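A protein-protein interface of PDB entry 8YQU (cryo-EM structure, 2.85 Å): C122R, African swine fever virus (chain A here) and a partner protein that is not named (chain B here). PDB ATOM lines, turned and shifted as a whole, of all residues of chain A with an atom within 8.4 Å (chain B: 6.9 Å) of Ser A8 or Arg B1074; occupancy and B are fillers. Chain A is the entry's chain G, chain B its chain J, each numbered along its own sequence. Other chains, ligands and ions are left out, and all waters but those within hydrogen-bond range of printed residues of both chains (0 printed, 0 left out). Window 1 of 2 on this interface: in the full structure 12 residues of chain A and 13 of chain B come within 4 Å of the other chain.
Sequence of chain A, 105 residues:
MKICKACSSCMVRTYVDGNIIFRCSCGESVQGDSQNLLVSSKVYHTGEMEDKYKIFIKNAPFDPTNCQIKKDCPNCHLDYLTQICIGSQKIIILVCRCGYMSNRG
Among the printed residues, pairs that only touch across the chains: Ser A8 with Arg B1074, Cys A26 with Tyr B1078, Cys A7 with Tyr B1078 and Ala A6 with Leu B1077.
The backbone carbonyl oxygen (O) of Lys A5 sits close to a ring nitrogen (NE2) of His B1123, at 3.3 Å.
A ring nitrogen (NE2) of His B1123 lies within hydrogen-bond range of the backbone carbonyl oxygen (O) of Ala A6, 2.9 Å away.
The backbone carbonyl oxygen of Cys A7 sits at hydrogen-bond distance from the guanidinium group of Arg B1074 (3.3 Å).
A ring nitrogen (ND1) of His B1123 lies close to the side-chain hydroxyl (OG) of Ser A8 (3.4 Å).
Of chain B, only Arg B1074 (3.3 Å) and His B1123 (3.4 Å) come within 4 Å of Ser A8.
Of chain A, only Cys A7 and Ser A8 come within 4 Å of Arg B1074.
Of the printed residues of chain A, Tyr B1078 touches Cys A7 (3.6 Å) and Cys A26 (3.6 Å).
Printed residues of chain B within 4 Å of Cys A7: Arg B1074 (3.3 Å) and Tyr B1078 (3.6 Å).
Printed residues of chain A within 4 Å of Leu B1077: Ala A6 (3.9 Å).
Of the printed residues of chain B, Ala A6 touches Leu B1077 and His B1123.
The nearest residue of chain B that does not touch Ser A8 is Lys B1127 (5.6 Å).
The nearest printed residue of chain B that does not touch Cys A7 is His B1123 (4.6 Å).
The side-chain sulfur (SG) of Cys A4 lies close to the backbone NH (N) of Ala A6, 3.5 Å away.
SG of Cys A7 lies close to OG of Ser A9 (3.3 Å).
The side-chain carboxylate of Asp B1070 lies within salt-bridge range of the guanidinium group of Arg B1074, 3.2 Å away.
Of the 19 printed residues of chain B, 4 touch a printed residue of chain A.
Hydrophobic or aromatic side chains of chain B within 4 Å of the printed part of chain A: Leu B1077, Tyr B1078 and His B1123.
Among the printed residues, no Asp or Glu carboxylate lies within 4 Å of a Lys or Arg side-chain nitrogen of the other chain.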
ATOM      1  N   MET A   1      -3.626  11.733 -10.610  1.00  0.00           N
ATOM      2  CA  MET A   1      -2.404  12.232  -9.988  1.00  0.00           C
ATOM      3  C   MET A   1      -1.260  12.274 -10.993  1.00  0.00           C
ATOM      4  O   MET A   1      -1.361  11.718 -12.087  1.00  0.00           O
ATOM      5  CB  MET A   1      -2.014  11.360  -8.795  1.00  0.00           C
ATOM      6  CG  MET A   1      -1.622   9.946  -9.180  1.00  0.00           C
ATOM      7  SD  MET A   1      -1.210   8.916  -7.762  1.00  0.00           S
ATOM      8  CE  MET A   1      -0.820   7.376  -8.585  1.00  0.00           C
ATOM      9  N   LYS A   2      -0.170  12.934 -10.614  1.00  0.00           N
ATOM     10  CA  LYS A   2       1.030  13.019 -11.436  1.00  0.00           C
ATOM     11  C   LYS A   2       2.157  12.275 -10.738  1.00  0.00           C
ATOM     12  O   LYS A   2       2.439  12.527  -9.561  1.00  0.00           O
ATOM     13  CB  LYS A   2       1.420  14.475 -11.692  1.00  0.00           C
ATOM     14  CG  LYS A   2       2.642  14.636 -12.579  1.00  0.00           C
ATOM     15  CD  LYS A   2       2.312  14.347 -14.033  1.00  0.00           C
ATOM     16  CE  LYS A   2       1.588  15.513 -14.681  1.00  0.00           C
ATOM     17  NZ  LYS A   2       1.429  15.313 -16.147  1.00  0.00           N
ATOM     18  N   ILE A   3       2.799  11.361 -11.461  1.00  0.00           N
ATOM     19  CA  ILE A   3       3.892  10.556 -10.935  1.00  0.00           C
ATOM     20  C   ILE A   3       5.207  11.153 -11.416  1.00  0.00           C
ATOM     21  O   ILE A   3       5.391  11.380 -12.618  1.00  0.00           O
ATOM     22  CB  ILE A   3       3.760   9.085 -11.366  1.00  0.00           C
ATOM     23  CG1 ILE A   3       2.650   8.395 -10.570  1.00  0.00           C
ATOM     24  CG2 ILE A   3       5.079   8.353 -11.190  1.00  0.00           C
ATOM     25  CD1 ILE A   3       2.899   8.354  -9.079  1.00  0.00           C
ATOM     26  N   CYS A   4       6.113  11.416 -10.477  1.00  0.00           N
ATOM     27  CA  CYS A   4       7.399  12.009 -10.814  1.00  0.00           C
ATOM     28  C   CYS A   4       8.186  11.095 -11.746  1.00  0.00           C
ATOM     29  O   CYS A   4       8.253   9.881 -11.544  1.00  0.00           O
ATOM     30  CB  CYS A   4       8.199  12.279  -9.539  1.00  0.00           C
ATOM     31  SG  CYS A   4       9.769  13.133  -9.789  1.00  0.00           S
ATOM     32  N   LYS A   5       8.771  11.688 -12.787  1.00  0.00           N
ATOM     33  CA  LYS A   5       9.601  10.912 -13.703  1.00  0.00           C
ATOM     34  C   LYS A   5      10.837  10.380 -12.985  1.00  0.00           C
ATOM     35  O   LYS A   5      11.201   9.210 -13.141  1.00  0.00           O
ATOM     36  CB  LYS A   5       9.977  11.782 -14.910  1.00  0.00           C
ATOM     37  CG  LYS A   5      11.197  11.376 -15.764  1.00  0.00           C
ATOM     38  CD  LYS A   5      11.287   9.883 -16.084  1.00  0.00           C
ATOM     39  CE  LYS A   5      10.115   9.411 -16.926  1.00  0.00           C
ATOM     40  NZ  LYS A   5      10.182   7.946 -17.182  1.00  0.00           N
ATOM     41  N   ALA A   6      11.469  11.216 -12.161  1.00  0.00           N
ATOM     42  CA  ALA A   6      12.735  10.850 -11.533  1.00  0.00           C
ATOM     43  C   ALA A   6      12.567   9.717 -10.525  1.00  0.00           C
ATOM     44  O   ALA A   6      13.137   8.633 -10.691  1.00  0.00           O
ATOM     45  CB  ALA A   6      13.352  12.078 -10.859  1.00  0.00           C
ATOM     46  N   CYS A   7      11.784   9.948  -9.472  1.00  0.00           N
ATOM     47  CA  CYS A   7      11.695   9.021  -8.353  1.00  0.00           C
ATOM     48  C   CYS A   7      10.368   8.277  -8.273  1.00  0.00           C
ATOM     49  O   CYS A   7      10.163   7.517  -7.321  1.00  0.00           O
ATOM     50  CB  CYS A   7      11.948   9.768  -7.039  1.00  0.00           C
ATOM     51  SG  CYS A   7      10.749  11.068  -6.687  1.00  0.00           S
ATOM     52  N   SER A   8       9.471   8.469  -9.242  1.00  0.00           N
ATOM     53  CA  SER A   8       8.182   7.770  -9.287  1.00  0.00           C
ATOM     54  C   SER A   8       7.383   7.969  -8.002  1.00  0.00           C
ATOM     55  O   SER A   8       6.758   7.040  -7.487  1.00  0.00           O
ATOM     56  CB  SER A   8       8.371   6.280  -9.582  1.00  0.00           C
ATOM     57  OG  SER A   8       8.923   6.084 -10.872  1.00  0.00           O
ATOM     58  N   SER A   9       7.399   9.189  -7.481  1.00  0.00           N
ATOM     59  CA  SER A   9       6.629   9.545  -6.300  1.00  0.00           C
ATOM     60  C   SER A   9       5.401  10.356  -6.695  1.00  0.00           C
ATOM     61  O   SER A   9       5.288  10.866  -7.812  1.00  0.00           O
ATOM     62  CB  SER A   9       7.492  10.326  -5.306  1.00  0.00           C
ATOM     63  OG  SER A   9       8.540   9.520  -4.796  1.00  0.00           O
ATOM     64  N   CYS A  10       4.469  10.471  -5.752  1.00  0.00           N
ATOM     65  CA  CYS A  10       3.237  11.223  -5.970  1.00  0.00           C
ATOM     66  C   CYS A  10       3.526  12.707  -5.783  1.00  0.00           C
ATOM     67  O   CYS A  10       3.763  13.165  -4.660  1.00  0.00           O
ATOM     68  CB  CYS A  10       2.147  10.748  -5.016  1.00  0.00           C
ATOM     69  SG  CYS A  10       0.583  11.627  -5.188  1.00  0.00           S
ATOM     70  N   MET A  11       3.507  13.459  -6.878  1.00  0.00           N
ATOM     71  CA  MET A  11       3.846  14.873  -6.838  1.00  0.00           C
ATOM     72  C   MET A  11       2.696  15.689  -6.256  1.00  0.00           C
ATOM     73  O   MET A  11       1.522  15.335  -6.394  1.00  0.00           O
ATOM     74  CB  MET A  11       4.196  15.371  -8.240  1.00  0.00           C
ATOM     75  CG  MET A  11       5.461  14.743  -8.802  1.00  0.00           C
ATOM     76  SD  MET A  11       5.847  15.257 -10.483  1.00  0.00           S
ATOM     77  CE  MET A  11       6.352  16.949 -10.205  1.00  0.00           C
ATOM     78  N   CYS A  24       7.579  18.043  -6.698  1.00  0.00           N
ATOM     79  CA  CYS A  24       7.883  16.813  -5.987  1.00  0.00           C
ATOM     80  C   CYS A  24       8.803  17.088  -4.803  1.00  0.00           C
ATOM     81  O   CYS A  24       9.353  18.179  -4.644  1.00  0.00           O
ATOM     82  CB  CYS A  24       8.522  15.794  -6.935  1.00  0.00           C
ATOM     83  SG  CYS A  24       8.732  14.150  -6.229  1.00  0.00           S
ATOM     84  N   CYS A  26      11.633  15.745  -4.456  1.00  0.00           N
ATOM     85  CA  CYS A  26      13.000  15.706  -4.954  1.00  0.00           C
ATOM     86  C   CYS A  26      13.364  16.951  -5.751  1.00  0.00           C
ATOM     87  O   CYS A  26      14.443  16.999  -6.350  1.00  0.00           O
ATOM     88  CB  CYS A  26      13.211  14.455  -5.809  1.00  0.00           C
ATOM     89  SG  CYS A  26      12.351  14.480  -7.396  1.00  0.00           S
ATOM     90  N   MET B1067      12.361  -5.828  -6.745  1.00  0.00           N
ATOM     91  CA  MET B1067      12.002  -4.607  -6.031  1.00  0.00           C
ATOM     92  C   MET B1067      13.178  -4.072  -5.226  1.00  0.00           C
ATOM     93  O   MET B1067      13.385  -2.854  -5.152  1.00  0.00           O
ATOM     94  CB  MET B1067      10.799  -4.863  -5.125  1.00  0.00           C
ATOM     95  CG  MET B1067       9.509  -5.174  -5.867  1.00  0.00           C
ATOM     96  SD  MET B1067       8.959  -3.804  -6.904  1.00  0.00           S
ATOM     97  CE  MET B1067       9.467  -4.357  -8.528  1.00  0.00           C
ATOM     98  N   VAL B1069      16.460  -4.285  -5.789  1.00  0.00           N
ATOM     99  CA  VAL B1069      17.427  -3.589  -6.632  1.00  0.00           C
ATOM    100  C   VAL B1069      16.829  -2.301  -7.182  1.00  0.00           C
ATOM    101  O   VAL B1069      17.506  -1.269  -7.257  1.00  0.00           O
ATOM    102  CB  VAL B1069      17.923  -4.508  -7.763  1.00  0.00           C
ATOM    103  CG1 VAL B1069      19.080  -3.854  -8.490  1.00  0.00           C
ATOM    104  CG2 VAL B1069      18.346  -5.852  -7.210  1.00  0.00           C
ATOM    105  N   ASP B1070      15.555  -2.341  -7.581  1.00  0.00           N
ATOM    106  CA  ASP B1070      14.910  -1.150  -8.124  1.00  0.00           C
ATOM    107  C   ASP B1070      14.812  -0.047  -7.079  1.00  0.00           C
ATOM    108  O   ASP B1070      14.942   1.139  -7.403  1.00  0.00           O
ATOM    109  CB  ASP B1070      13.526  -1.504  -8.665  1.00  0.00           C
ATOM    110  CG  ASP B1070      12.722  -0.280  -9.046  1.00  0.00           C
ATOM    111  OD1 ASP B1070      13.093   0.394 -10.029  1.00  0.00           O
ATOM    112  OD2 ASP B1070      11.719   0.011  -8.359  1.00  0.00           O
ATOM    113  N   SER B1071      14.572  -0.418  -5.820  1.00  0.00           N
ATOM    114  CA  SER B1071      14.524   0.577  -4.754  1.00  0.00           C
ATOM    115  C   SER B1071      15.870   1.266  -4.585  1.00  0.00           C
ATOM    116  O   SER B1071      15.931   2.476  -4.336  1.00  0.00           O
ATOM    117  CB  SER B1071      14.089  -0.078  -3.443  1.00  0.00           C
ATOM    118  OG  SER B1071      14.060   0.866  -2.387  1.00  0.00           O
ATOM    119  N   ALA B1072      16.964   0.511  -4.712  1.00  0.00           N
ATOM    120  CA  ALA B1072      18.290   1.111  -4.615  1.00  0.00           C
ATOM    121  C   ALA B1072      18.551   2.065  -5.773  1.00  0.00           C
ATOM    122  O   ALA B1072      19.251   3.072  -5.613  1.00  0.00           O
ATOM    123  CB  ALA B1072      19.358   0.019  -4.568  1.00  0.00           C
ATOM    124  N   VAL B1073      18.009   1.760  -6.954  1.00  0.00           N
ATOM    125  CA  VAL B1073      18.216   2.628  -8.108  1.00  0.00           C
ATOM    126  C   VAL B1073      17.507   3.964  -7.913  1.00  0.00           C
ATOM    127  O   VAL B1073      18.074   5.028  -8.186  1.00  0.00           O
ATOM    128  CB  VAL B1073      17.756   1.927  -9.399  1.00  0.00           C
ATOM    129  CG1 VAL B1073      17.852   2.877 -10.580  1.00  0.00           C
ATOM    130  CG2 VAL B1073      18.589   0.684  -9.652  1.00  0.00           C
ATOM    131  N   ARG B1074      16.262   3.934  -7.435  1.00  0.00           N
ATOM    132  CA  ARG B1074      15.473   5.157  -7.361  1.00  0.00           C
ATOM    133  C   ARG B1074      15.898   6.081  -6.228  1.00  0.00           C
ATOM    134  O   ARG B1074      15.603   7.279  -6.293  1.00  0.00           O
ATOM    135  CB  ARG B1074      13.985   4.834  -7.219  1.00  0.00           C
ATOM    136  CG  ARG B1074      13.591   4.223  -5.891  1.00  0.00           C
ATOM    137  CD  ARG B1074      12.100   3.941  -5.856  1.00  0.00           C
ATOM    138  NE  ARG B1074      11.714   2.921  -6.823  1.00  0.00           N
ATOM    139  CZ  ARG B1074      11.040   3.167  -7.937  1.00  0.00           C
ATOM    140  NH1 ARG B1074      10.672   4.394  -8.264  1.00  0.00           N
ATOM    141  NH2 ARG B1074      10.731   2.157  -8.745  1.00  0.00           N
ATOM    142  N   ILE B1075      16.577   5.573  -5.198  1.00  0.00           N
ATOM    143  CA  ILE B1075      17.130   6.459  -4.180  1.00  0.00           C
ATOM    144  C   ILE B1075      18.417   7.120  -4.654  1.00  0.00           C
ATOM    145  O   ILE B1075      18.757   8.211  -4.173  1.00  0.00           O
ATOM    146  CB  ILE B1075      17.365   5.718  -2.850  1.00  0.00           C
ATOM    147  CG1 ILE B1075      18.474   4.676  -2.990  1.00  0.00           C
ATOM    148  CG2 ILE B1075      16.077   5.070  -2.366  1.00  0.00           C
ATOM    149  CD1 ILE B1075      18.873   4.042  -1.679  1.00  0.00           C
ATOM    150  N   PHE B1076      19.144   6.494  -5.582  1.00  0.00           N
ATOM    151  CA  PHE B1076      20.216   7.197  -6.277  1.00  0.00           C
ATOM    152  C   PHE B1076      19.651   8.332  -7.120  1.00  0.00           C
ATOM    153  O   PHE B1076      20.210   9.433  -7.146  1.00  0.00           O
ATOM    154  CB  PHE B1076      21.005   6.214  -7.143  1.00  0.00           C
ATOM    155  CG  PHE B1076      22.370   6.706  -7.545  1.00  0.00           C
ATOM    156  CD1 PHE B1076      22.514   7.756  -8.436  1.00  0.00           C
ATOM    157  CD2 PHE B1076      23.509   6.114  -7.029  1.00  0.00           C
ATOM    158  CE1 PHE B1076      23.767   8.206  -8.802  1.00  0.00           C
ATOM    159  CE2 PHE B1076      24.765   6.559  -7.392  1.00  0.00           C
ATOM    160  CZ  PHE B1076      24.894   7.606  -8.280  1.00  0.00           C
ATOM    161  N   LEU B1077      18.537   8.079  -7.810  1.00  0.00           N
ATOM    162  CA  LEU B1077      17.919   9.109  -8.638  1.00  0.00           C
ATOM    163  C   LEU B1077      17.242  10.175  -7.785  1.00  0.00           C
ATOM    164  O   LEU B1077      17.286  11.364  -8.121  1.00  0.00           O
ATOM    165  CB  LEU B1077      16.918   8.466  -9.595  1.00  0.00           C
ATOM    166  CG  LEU B1077      17.513   7.409 -10.526  1.00  0.00           C
ATOM    167  CD1 LEU B1077      16.419   6.610 -11.211  1.00  0.00           C
ATOM    168  CD2 LEU B1077      18.429   8.058 -11.549  1.00  0.00           C
ATOM    169  N   TYR B1078      16.603   9.769  -6.686  1.00  0.00           N
ATOM    170  CA  TYR B1078      15.939  10.731  -5.811  1.00  0.00           C
ATOM    171  C   TYR B1078      16.943  11.696  -5.194  1.00  0.00           C
ATOM    172  O   TYR B1078      16.703  12.908  -5.136  1.00  0.00           O
ATOM    173  CB  TYR B1078      15.160   9.991  -4.721  1.00  0.00           C
ATOM    174  CG  TYR B1078      14.449  10.894  -3.740  1.00  0.00           C
ATOM    175  CD1 TYR B1078      13.183  11.389  -4.016  1.00  0.00           C
ATOM    176  CD2 TYR B1078      15.039  11.242  -2.533  1.00  0.00           C
ATOM    177  CE1 TYR B1078      12.527  12.211  -3.120  1.00  0.00           C
ATOM    178  CE2 TYR B1078      14.392  12.064  -1.631  1.00  0.00           C
ATOM    179  CZ  TYR B1078      13.137  12.545  -1.930  1.00  0.00           C
ATOM    180  OH  TYR B1078      12.487  13.362  -1.036  1.00  0.00           O
ATOM    181  N   ASN B1079      18.079  11.174  -4.726  1.00  0.00           N
ATOM    182  CA  ASN B1079      19.076  12.031  -4.097  1.00  0.00           C
ATOM    183  C   ASN B1079      19.840  12.858  -5.123  1.00  0.00           C
ATOM    184  O   ASN B1079      20.251  13.985  -4.824  1.00  0.00           O
ATOM    185  CB  ASN B1079      20.043  11.187  -3.268  1.00  0.00           C
ATOM    186  CG  ASN B1079      19.413  10.670  -1.991  1.00  0.00           C
ATOM    187  OD1 ASN B1079      18.624  11.364  -1.350  1.00  0.00           O
ATOM    188  ND2 ASN B1079      19.760   9.445  -1.614  1.00  0.00           N
ATOM    189  N   TYR B1080      20.046  12.319  -6.326  1.00  0.00           N
ATOM    190  CA  TYR B1080      20.730  13.080  -7.366  1.00  0.00           C
ATOM    191  C   TYR B1080      19.911  14.291  -7.791  1.00  0.00           C
ATOM    192  O   TYR B1080      20.466  15.372  -8.025  1.00  0.00           O
ATOM    193  CB  TYR B1080      21.027  12.183  -8.566  1.00  0.00           C
ATOM    194  CG  TYR B1080      21.565  12.923  -9.767  1.00  0.00           C
ATOM    195  CD1 TYR B1080      22.769  13.612  -9.699  1.00  0.00           C
ATOM    196  CD2 TYR B1080      20.875  12.929 -10.970  1.00  0.00           C
ATOM    197  CE1 TYR B1080      23.266  14.288 -10.794  1.00  0.00           C
ATOM    198  CE2 TYR B1080      21.365  13.602 -12.072  1.00  0.00           C
ATOM    199  CZ  TYR B1080      22.561  14.280 -11.977  1.00  0.00           C
ATOM    200  OH  TYR B1080      23.055  14.952 -13.071  1.00  0.00           O
ATOM    201  N   TYR B1122      14.793   4.586 -17.632  1.00  0.00           N
ATOM    202  CA  TYR B1122      14.936   3.464 -16.708  1.00  0.00           C
ATOM    203  C   TYR B1122      13.587   2.860 -16.342  1.00  0.00           C
ATOM    204  O   TYR B1122      13.383   1.649 -16.483  1.00  0.00           O
ATOM    205  CB  TYR B1122      15.667   3.901 -15.440  1.00  0.00           C
ATOM    206  CG  TYR B1122      15.574   2.873 -14.335  1.00  0.00           C
ATOM    207  CD1 TYR B1122      16.186   1.633 -14.463  1.00  0.00           C
ATOM    208  CD2 TYR B1122      14.862   3.135 -13.173  1.00  0.00           C
ATOM    209  CE1 TYR B1122      16.099   0.687 -13.461  1.00  0.00           C
ATOM    210  CE2 TYR B1122      14.768   2.194 -12.166  1.00  0.00           C
ATOM    211  CZ  TYR B1122      15.389   0.973 -12.315  1.00  0.00           C
ATOM    212  OH  TYR B1122      15.300   0.033 -11.314  1.00  0.00           O
ATOM    213  N   HIS B1123      12.659   3.689 -15.859  1.00  0.00           N
ATOM    214  CA  HIS B1123      11.413   3.172 -15.302  1.00  0.00           C
ATOM    215  C   HIS B1123      10.586   2.445 -16.356  1.00  0.00           C
ATOM    216  O   HIS B1123       9.994   1.397 -16.074  1.00  0.00           O
ATOM    217  CB  HIS B1123      10.612   4.313 -14.678  1.00  0.00           C
ATOM    218  CG  HIS B1123      11.296   4.962 -13.514  1.00  0.00           C
ATOM    219  ND1 HIS B1123      11.482   4.322 -12.309  1.00  0.00           N
ATOM    220  CD2 HIS B1123      11.842   6.192 -13.375  1.00  0.00           C
ATOM    221  CE1 HIS B1123      12.110   5.131 -11.474  1.00  0.00           C
ATOM    222  NE2 HIS B1123      12.341   6.272 -12.097  1.00  0.00           N
ATOM    223  N   PHE B1126      12.389  -0.984 -17.130  1.00  0.00           N
ATOM    224  CA  PHE B1126      12.362  -1.932 -16.019  1.00  0.00           C
ATOM    225  C   PHE B1126      10.995  -2.589 -15.881  1.00  0.00           C
ATOM    226  O   PHE B1126      10.901  -3.800 -15.646  1.00  0.00           O
ATOM    227  CB  PHE B1126      12.752  -1.235 -14.718  1.00  0.00           C
ATOM    228  CG  PHE B1126      12.588  -2.097 -13.500  1.00  0.00           C
ATOM    229  CD1 PHE B1126      13.457  -3.145 -13.258  1.00  0.00           C
ATOM    230  CD2 PHE B1126      11.562  -1.863 -12.601  1.00  0.00           C
ATOM    231  CE1 PHE B1126      13.310  -3.942 -12.140  1.00  0.00           C
ATOM    232  CE2 PHE B1126      11.409  -2.657 -11.482  1.00  0.00           C
ATOM    233  CZ  PHE B1126      12.284  -3.698 -11.252  1.00  0.00           C
ATOM    234  N   LYS B1127       9.922  -1.806 -16.015  1.00  0.00           N
ATOM    235  CA  LYS B1127       8.581  -2.371 -15.914  1.00  0.00           C
ATOM    236  C   LYS B1127       8.294  -3.343 -17.051  1.00  0.00           C
ATOM    237  O   LYS B1127       7.538  -4.304 -16.866  1.00  0.00           O
ATOM    238  CB  LYS B1127       7.541  -1.252 -15.886  1.00  0.00           C
ATOM    239  CG  LYS B1127       7.567  -0.427 -14.611  1.00  0.00           C
ATOM    240  CD  LYS B1127       6.462   0.615 -14.595  1.00  0.00           C
ATOM    241  CE  LYS B1127       6.520   1.453 -13.328  1.00  0.00           C
ATOM    242  NZ  LYS B1127       5.419   2.453 -13.266  1.00  0.00           N
ATOM    243  N   LEU B1145      22.595   1.206 -12.438  1.00  0.00           N
ATOM    244  CA  LEU B1145      23.207   1.912 -11.318  1.00  0.00           C
ATOM    245  C   LEU B1145      24.687   2.172 -11.571  1.00  0.00           C
ATOM    246  O   LEU B1145      25.211   3.227 -11.194  1.00  0.00           O
ATOM    247  CB  LEU B1145      23.015   1.118 -10.028  1.00  0.00           C
ATOM    248  CG  LEU B1145      23.266   1.879  -8.727  1.00  0.00           C
ATOM    249  CD1 LEU B1145      22.275   3.021  -8.583  1.00  0.00           C
ATOM    250  CD2 LEU B1145      23.187   0.941  -7.535  1.00  0.00           C
ATOM    251  N   ILE B1176      24.205   3.418  -0.568  1.00  0.00           N
ATOM    252  CA  ILE B1176      23.355   2.365  -1.116  1.00  0.00           C
ATOM    253  C   ILE B1176      23.915   0.995  -0.755  1.00  0.00           C
ATOM    254  O   ILE B1176      23.180   0.092  -0.336  1.00  0.00           O
ATOM    255  CB  ILE B1176      23.213   2.534  -2.640  1.00  0.00           C
ATOM    256  CG1 ILE B1176      22.243   3.673  -2.958  1.00  0.00           C
ATOM    257  CG2 ILE B1176      22.748   1.238  -3.287  1.00  0.00           C
ATOM    258  CD1 ILE B1176      22.179   4.026  -4.422  1.00  0.00           C
